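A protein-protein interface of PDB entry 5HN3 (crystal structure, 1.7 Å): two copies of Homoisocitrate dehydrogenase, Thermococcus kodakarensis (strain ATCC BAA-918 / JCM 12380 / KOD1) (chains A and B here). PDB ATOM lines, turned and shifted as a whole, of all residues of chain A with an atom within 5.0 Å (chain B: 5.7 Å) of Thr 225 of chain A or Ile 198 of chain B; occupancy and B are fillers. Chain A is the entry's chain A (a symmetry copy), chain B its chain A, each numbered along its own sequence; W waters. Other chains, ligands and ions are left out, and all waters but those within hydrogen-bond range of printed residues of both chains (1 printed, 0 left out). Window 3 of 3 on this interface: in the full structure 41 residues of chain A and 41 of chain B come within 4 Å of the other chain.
No position is printed for both chains.
Of the 9 pairs that touch across the chains among the printed residues, none has its exchanged pair printed and touching as well.
Asp 222 of chain A touches Asp 194 of chain B.
Asp 222 of chain A touches Ser 195 of chain B.
CG1 of Ile 198 of chain B touches O of Asp 222 of chain A, 3.5 Å away.
Thr 197 of chain B touches Leu 223 of chain A.
Val 201 of chain B touches Leu 223 of chain A.
Thr 225 of chain A touches Ile 198 of chain B.
Thr 225 of chain A touches Arg 202 of chain B (O to NH2, 3.8 Å).
Of the 12 printed residues of chain A, 5 touch a printed residue of chain B.
Hydrophobic or aromatic side chains of chain A that line the printed part of chain B: Leu 223.
Hydrophobic or aromatic side chains of chain B that line the printed part of chain A: Ile 198 and Val 201.
Among the printed residues, no Asp or Glu carboxylate lies within 4 Å of a Lys or Arg side-chain nitrogen of the other chain.
O of Asp 194 of chain B lies within hydrogen-bond range of OG1 of Thr 197 of chain B, at 2.8 Å.
The guanidinium group (NH2) of Arg 96 of chain A lies within salt-bridge range of the side-chain carboxylate (OD1) of Asp 222 of chain A (3.1 Å).
OG1 of Thr 225 of chain A lies within hydrogen-bond range of O of Asp 222 of chain A, 2.7 Å away.
Ser 221 of chain A touches none of the printed residues of chain B.
Printed residues of chain B within 4 Å of Asp 222 of chain A: Asp 194, Ser 195 and Ile 198.
Thr 225 of chain A touches just these residues of chain B: Ile 198 (3.5 Å) and Arg 202 (3.8 Å).
Of the printed residues of chain B, Val 226 of chain A touches Arg 202.
Of the printed residues of chain A, Ile 198 of chain B touches Asp 222 and Thr 225.
Asn 203 of chain B touches none of the printed residues of chain A.
Water W1 lies within hydrogen-bond range of the side-chain carboxylate of Asp 194 of chain B (2.8 Å) and the side-chain carboxylate of Asp 222 of chain A (2.8 Å).
The guanidinium group of Arg 202 of chain B lies within hydrogen-bond range of the backbone carbonyl oxygen of Val 226 of chain A.
The guanidinium group (NH2) of Arg 202 of chain B sits at hydrogen-bond distance from the backbone carbonyl oxygen (O) of Ala 228 of chain A (3.4 Å).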
ATOM      1  N   ARG A  96       4.530   3.308 -20.565  1.00  0.00           N
ATOM      2  CA  ARG A  96       4.666   1.866 -20.743  1.00  0.00           C
ATOM      3  C   ARG A  96       4.652   1.559 -22.229  1.00  0.00           C
ATOM      4  O   ARG A  96       3.841   2.151 -22.987  1.00  0.00           O
ATOM      5  CB  ARG A  96       3.500   1.088 -20.130  1.00  0.00           C
ATOM      6  CG  ARG A  96       3.714  -0.432 -20.099  1.00  0.00           C
ATOM      7  CD  ARG A  96       2.557  -1.161 -19.442  1.00  0.00           C
ATOM      8  NE  ARG A  96       2.556  -0.940 -18.003  1.00  0.00           N
ATOM      9  CZ  ARG A  96       1.888  -1.658 -17.135  1.00  0.00           C
ATOM     10  NH1 ARG A  96       2.021  -1.410 -15.839  1.00  0.00           N
ATOM     11  NH2 ARG A  96       1.030  -2.582 -17.559  1.00  0.00           N
ATOM     12  N   ILE A  98       4.154  -1.646 -24.919  1.00  0.00           N
ATOM     13  CA  ILE A  98       3.961  -3.074 -25.247  1.00  0.00           C
ATOM     14  C   ILE A  98       4.527  -3.223 -26.657  1.00  0.00           C
ATOM     15  O   ILE A  98       3.989  -2.683 -27.613  1.00  0.00           O
ATOM     16  CB  ILE A  98       2.486  -3.528 -25.172  1.00  0.00           C
ATOM     17  CG1 ILE A  98       1.980  -3.619 -23.705  1.00  0.00           C
ATOM     18  CG2 ILE A  98       2.352  -4.932 -25.765  1.00  0.00           C
ATOM     19  CD1 ILE A  98       2.089  -2.432 -22.825  1.00  0.00           C
ATOM     20  N   SER A 221      -3.159   0.214 -19.694  1.00  0.00           N
ATOM     21  CA  SER A 221      -1.757  -0.246 -19.694  1.00  0.00           C
ATOM     22  C   SER A 221      -1.680  -1.741 -19.380  1.00  0.00           C
ATOM     23  O   SER A 221      -0.760  -2.437 -19.913  1.00  0.00           O
ATOM     24  CB  SER A 221      -0.919   0.616 -18.729  1.00  0.00           C
ATOM     25  OG  SER A 221      -1.310   0.391 -17.441  1.00  0.00           O
ATOM     26  N   ASP A 222      -2.613  -2.273 -18.604  1.00  0.00           N
ATOM     27  CA  ASP A 222      -2.762  -3.733 -18.370  1.00  0.00           C
ATOM     28  C   ASP A 222      -3.452  -4.408 -19.529  1.00  0.00           C
ATOM     29  O   ASP A 222      -2.954  -5.429 -20.009  1.00  0.00           O
ATOM     30  CB  ASP A 222      -3.478  -4.051 -17.063  1.00  0.00           C
ATOM     31  CG  ASP A 222      -2.550  -3.864 -15.808  1.00  0.00           C
ATOM     32  OD1 ASP A 222      -1.324  -3.777 -15.982  1.00  0.00           O
ATOM     33  OD2 ASP A 222      -3.053  -3.826 -14.683  1.00  0.00           O
ATOM     34  N   LEU A 223      -4.578  -3.862 -19.976  1.00  0.00           N
ATOM     35  CA  LEU A 223      -5.278  -4.480 -21.110  1.00  0.00           C
ATOM     36  C   LEU A 223      -4.304  -4.655 -22.348  1.00  0.00           C
ATOM     37  O   LEU A 223      -4.353  -5.682 -23.028  1.00  0.00           O
ATOM     38  CB  LEU A 223      -6.506  -3.699 -21.504  1.00  0.00           C
ATOM     39  CG  LEU A 223      -7.251  -4.165 -22.748  1.00  0.00           C
ATOM     40  CD1 LEU A 223      -7.688  -5.631 -22.674  1.00  0.00           C
ATOM     41  CD2 LEU A 223      -8.443  -3.260 -22.990  1.00  0.00           C
ATOM     42  N   ALA A 224      -3.477  -3.657 -22.622  1.00  0.00           N
ATOM     43  CA  ALA A 224      -2.535  -3.676 -23.762  1.00  0.00           C
ATOM     44  C   ALA A 224      -1.609  -4.889 -23.716  1.00  0.00           C
ATOM     45  O   ALA A 224      -1.162  -5.331 -24.774  1.00  0.00           O
ATOM     46  CB  ALA A 224      -1.720  -2.382 -23.799  1.00  0.00           C
ATOM     47  N   THR A 225      -1.350  -5.417 -22.527  1.00  0.00           N
ATOM     48  CA  THR A 225      -0.452  -6.586 -22.356  1.00  0.00           C
ATOM     49  C   THR A 225      -0.989  -7.867 -22.899  1.00  0.00           C
ATOM     50  O   THR A 225      -0.219  -8.864 -23.017  1.00  0.00           O
ATOM     51  CB  THR A 225       0.019  -6.814 -20.901  1.00  0.00           C
ATOM     52  OG1 THR A 225      -1.008  -7.336 -20.077  1.00  0.00           O
ATOM     53  CG2 THR A 225       0.673  -5.561 -20.308  1.00  0.00           C
ATOM     54  N   VAL A 226      -2.261  -7.909 -23.280  1.00  0.00           N
ATOM     55  CA  VAL A 226      -2.740  -9.091 -24.006  1.00  0.00           C
ATOM     56  C   VAL A 226      -1.998  -9.333 -25.302  1.00  0.00           C
ATOM     57  O   VAL A 226      -2.028 -10.477 -25.796  1.00  0.00           O
ATOM     58  CB  VAL A 226      -4.243  -9.153 -24.272  1.00  0.00           C
ATOM     59  CG1 VAL A 226      -5.011  -9.024 -22.969  1.00  0.00           C
ATOM     60  CG2 VAL A 226      -4.712  -8.135 -25.304  1.00  0.00           C
ATOM     61  N   HIS A 227      -1.364  -8.293 -25.835  1.00  0.00           N
ATOM     62  CA  HIS A 227      -0.578  -8.409 -27.070  1.00  0.00           C
ATOM     63  C   HIS A 227       0.852  -8.735 -26.856  1.00  0.00           C
ATOM     64  O   HIS A 227       1.610  -8.763 -27.835  1.00  0.00           O
ATOM     65  CB  HIS A 227      -0.685  -7.137 -27.880  1.00  0.00           C
ATOM     66  CG  HIS A 227      -2.082  -6.799 -28.182  1.00  0.00           C
ATOM     67  ND1 HIS A 227      -2.835  -7.552 -29.046  1.00  0.00           N
ATOM     68  CD2 HIS A 227      -2.893  -5.807 -27.726  1.00  0.00           C
ATOM     69  CE1 HIS A 227      -4.058  -7.058 -29.102  1.00  0.00           C
ATOM     70  NE2 HIS A 227      -4.112  -5.991 -28.326  1.00  0.00           N
ATOM     71  N   ALA A 228       1.236  -8.968 -25.614  1.00  0.00           N
ATOM     72  CA  ALA A 228       2.599  -9.411 -25.304  1.00  0.00           C
ATOM     73  C   ALA A 228       2.544 -10.891 -24.962  1.00  0.00           C
ATOM     74  O   ALA A 228       1.638 -11.341 -24.270  1.00  0.00           O
ATOM     75  CB  ALA A 228       3.136  -8.613 -24.137  1.00  0.00           C
ATOM     76  N   ILE A 231       4.565 -10.767 -19.789  1.00  0.00           N
ATOM     77  CA  ILE A 231       4.879  -9.496 -19.164  1.00  0.00           C
ATOM     78  C   ILE A 231       6.364  -9.265 -19.118  1.00  0.00           C
ATOM     79  O   ILE A 231       6.781  -8.149 -19.082  1.00  0.00           O
ATOM     80  CB  ILE A 231       4.255  -9.390 -17.753  1.00  0.00           C
ATOM     81  CG1 ILE A 231       4.136  -7.975 -17.263  1.00  0.00           C
ATOM     82  CG2 ILE A 231       5.022 -10.203 -16.740  1.00  0.00           C
ATOM     83  CD1 ILE A 231       3.226  -7.057 -18.049  1.00  0.00           C
ATOM     84  N   VAL A 234       8.102  -6.365 -21.344  1.00  0.00           N
ATOM     85  CA  VAL A 234       7.530  -5.042 -21.378  1.00  0.00           C
ATOM     86  C   VAL A 234       8.371  -4.042 -20.617  1.00  0.00           C
ATOM     87  O   VAL A 234       8.541  -4.171 -19.355  1.00  0.00           O
ATOM     88  CB  VAL A 234       6.085  -5.122 -20.826  1.00  0.00           C
ATOM     89  CG1 VAL A 234       5.494  -3.729 -20.751  1.00  0.00           C
ATOM     90  CG2 VAL A 234       5.273  -6.035 -21.702  1.00  0.00           C
ATOM     91  N   ILE B 193     -10.406  -3.860 -11.695  1.00  0.00           N
ATOM     92  CA  ILE B 193     -10.679  -3.793 -13.166  1.00  0.00           C
ATOM     93  C   ILE B 193      -9.413  -3.908 -14.051  1.00  0.00           C
ATOM     94  O   ILE B 193      -9.426  -4.647 -15.053  1.00  0.00           O
ATOM     95  CB  ILE B 193     -11.523  -2.586 -13.611  1.00  0.00           C
ATOM     96  CG1 ILE B 193     -11.858  -2.747 -15.124  1.00  0.00           C
ATOM     97  CG2 ILE B 193     -10.867  -1.251 -13.283  1.00  0.00           C
ATOM     98  CD1 ILE B 193     -13.074  -2.036 -15.595  1.00  0.00           C
ATOM     99  N   ASP B 194      -8.301  -3.235 -13.699  1.00  0.00           N
ATOM    100  CA  ASP B 194      -7.133  -3.169 -14.518  1.00  0.00           C
ATOM    101  C   ASP B 194      -6.701  -4.575 -14.997  1.00  0.00           C
ATOM    102  O   ASP B 194      -6.649  -4.818 -16.189  1.00  0.00           O
ATOM    103  CB  ASP B 194      -5.944  -2.534 -13.789  1.00  0.00           C
ATOM    104  CG  ASP B 194      -6.218  -1.174 -13.194  1.00  0.00           C
ATOM    105  OD1 ASP B 194      -7.380  -0.736 -13.122  1.00  0.00           O
ATOM    106  OD2 ASP B 194      -5.200  -0.547 -12.747  1.00  0.00           O
ATOM    107  N   SER B 195      -6.436  -5.454 -14.035  1.00  0.00           N
ATOM    108  CA  SER B 195      -6.028  -6.864 -14.317  1.00  0.00           C
ATOM    109  C   SER B 195      -7.179  -7.711 -14.811  1.00  0.00           C
ATOM    110  O   SER B 195      -6.961  -8.666 -15.591  1.00  0.00           O
ATOM    111  CB  SER B 195      -5.371  -7.503 -13.086  1.00  0.00           C
ATOM    112  OG  SER B 195      -6.178  -7.391 -11.926  1.00  0.00           O
ATOM    113  N   PHE B 196      -8.400  -7.427 -14.361  1.00  0.00           N
ATOM    114  CA  PHE B 196      -9.553  -8.204 -14.797  1.00  0.00           C
ATOM    115  C   PHE B 196      -9.767  -8.116 -16.323  1.00  0.00           C
ATOM    116  O   PHE B 196     -10.204  -9.104 -16.968  1.00  0.00           O
ATOM    117  CB  PHE B 196     -10.854  -7.793 -14.086  1.00  0.00           C
ATOM    118  CG  PHE B 196     -11.987  -8.716 -14.405  1.00  0.00           C
ATOM    119  CD1 PHE B 196     -12.010  -9.988 -13.847  1.00  0.00           C
ATOM    120  CD2 PHE B 196     -12.960  -8.342 -15.322  1.00  0.00           C
ATOM    121  CE1 PHE B 196     -13.035 -10.882 -14.194  1.00  0.00           C
ATOM    122  CE2 PHE B 196     -13.961  -9.217 -15.663  1.00  0.00           C
ATOM    123  CZ  PHE B 196     -13.992 -10.469 -15.082  1.00  0.00           C
ATOM    124  N   THR B 197      -9.442  -6.986 -16.904  1.00  0.00           N
ATOM    125  CA  THR B 197      -9.607  -6.835 -18.355  1.00  0.00           C
ATOM    126  C   THR B 197      -8.846  -7.910 -19.122  1.00  0.00           C
ATOM    127  O   THR B 197      -9.344  -8.369 -20.171  1.00  0.00           O
ATOM    128  CB  THR B 197      -9.234  -5.471 -18.922  1.00  0.00           C
ATOM    129  OG1 THR B 197      -7.841  -5.173 -18.725  1.00  0.00           O
ATOM    130  CG2 THR B 197     -10.153  -4.380 -18.364  1.00  0.00           C
ATOM    131  N   ILE B 198      -7.689  -8.276 -18.629  1.00  0.00           N
ATOM    132  CA  ILE B 198      -6.871  -9.355 -19.267  1.00  0.00           C
ATOM    133  C   ILE B 198      -7.653 -10.691 -19.222  1.00  0.00           C
ATOM    134  O   ILE B 198      -7.741 -11.460 -20.218  1.00  0.00           O
ATOM    135  CB  ILE B 198      -5.494  -9.457 -18.608  1.00  0.00           C
ATOM    136  CG1 ILE B 198      -4.688  -8.170 -18.788  1.00  0.00           C
ATOM    137  CG2 ILE B 198      -4.699 -10.681 -19.150  1.00  0.00           C
ATOM    138  CD1 ILE B 198      -3.561  -8.051 -17.789  1.00  0.00           C
ATOM    139  N   LYS B 199      -8.276 -10.988 -18.073  1.00  0.00           N
ATOM    140  CA  LYS B 199      -9.033 -12.216 -17.912  1.00  0.00           C
ATOM    141  C   LYS B 199     -10.278 -12.209 -18.777  1.00  0.00           C
ATOM    142  O   LYS B 199     -10.682 -13.257 -19.320  1.00  0.00           O
ATOM    143  CB  LYS B 199      -9.414 -12.431 -16.448  1.00  0.00           C
ATOM    144  CG  LYS B 199      -8.227 -12.539 -15.499  1.00  0.00           C
ATOM    145  CD  LYS B 199      -8.705 -12.869 -14.088  1.00  0.00           C
ATOM    146  CE  LYS B 199      -7.567 -13.372 -13.210  1.00  0.00           C
ATOM    147  NZ  LYS B 199      -6.470 -12.378 -13.125  1.00  0.00           N
ATOM    148  N   LEU B 200     -10.908 -11.023 -18.942  1.00  0.00           N
ATOM    149  CA  LEU B 200     -12.095 -10.957 -19.766  1.00  0.00           C
ATOM    150  C   LEU B 200     -11.778 -11.165 -21.264  1.00  0.00           C
ATOM    151  O   LEU B 200     -12.598 -11.771 -21.991  1.00  0.00           O
ATOM    152  CB  LEU B 200     -12.805  -9.636 -19.561  1.00  0.00           C
ATOM    153  CG  LEU B 200     -14.085  -9.429 -20.316  1.00  0.00           C
ATOM    154  CD1 LEU B 200     -15.130 -10.478 -19.956  1.00  0.00           C
ATOM    155  CD2 LEU B 200     -14.660  -8.056 -19.951  1.00  0.00           C
ATOM    156  N   VAL B 201     -10.581 -10.798 -21.691  1.00  0.00           N
ATOM    157  CA  VAL B 201     -10.146 -11.081 -23.076  1.00  0.00           C
ATOM    158  C   VAL B 201      -9.752 -12.564 -23.224  1.00  0.00           C
ATOM    159  O   VAL B 201     -10.164 -13.217 -24.211  1.00  0.00           O
ATOM    160  CB  VAL B 201      -8.946 -10.193 -23.475  1.00  0.00           C
ATOM    161  CG1 VAL B 201      -8.343 -10.618 -24.810  1.00  0.00           C
ATOM    162  CG2 VAL B 201      -9.390  -8.754 -23.526  1.00  0.00           C
ATOM    163  N   ARG B 202      -8.978 -13.078 -22.275  1.00  0.00           N
ATOM    164  CA  ARG B 202      -8.334 -14.416 -22.401  1.00  0.00           C
ATOM    165  C   ARG B 202      -9.228 -15.568 -21.971  1.00  0.00           C
ATOM    166  O   ARG B 202      -9.172 -16.660 -22.603  1.00  0.00           O
ATOM    167  CB  ARG B 202      -6.988 -14.448 -21.669  1.00  0.00           C
ATOM    168  CG  ARG B 202      -5.961 -13.597 -22.356  1.00  0.00           C
ATOM    169  CD  ARG B 202      -4.571 -13.733 -21.786  1.00  0.00           C
ATOM    170  NE  ARG B 202      -3.574 -13.217 -22.721  1.00  0.00           N
ATOM    171  CZ  ARG B 202      -2.343 -12.834 -22.379  1.00  0.00           C
ATOM    172  NH1 ARG B 202      -1.942 -12.895 -21.112  1.00  0.00           N
ATOM    173  NH2 ARG B 202      -1.500 -12.405 -23.322  1.00  0.00           N
ATOM    174  N   ASN B 203     -10.069 -15.374 -20.960  1.00  0.00           N
ATOM    175  CA  ASN B 203     -10.913 -16.417 -20.395  1.00  0.00           C
ATOM    176  C   ASN B 203     -12.324 -15.873 -20.091  1.00  0.00           C
ATOM    177  O   ASN B 203     -12.742 -15.786 -18.955  1.00  0.00           O
ATOM    178  CB  ASN B 203     -10.239 -16.995 -19.111  1.00  0.00           C
ATOM    179  CG  ASN B 203     -11.024 -18.140 -18.486  1.00  0.00           C
ATOM    180  OD1 ASN B 203     -11.639 -18.931 -19.193  1.00  0.00           O
ATOM    181  ND2 ASN B 203     -10.973 -18.257 -17.144  1.00  0.00           N
HETATM  182  O   HOH W   1      -2.653  -1.546 -13.123  1.00  0.00           O
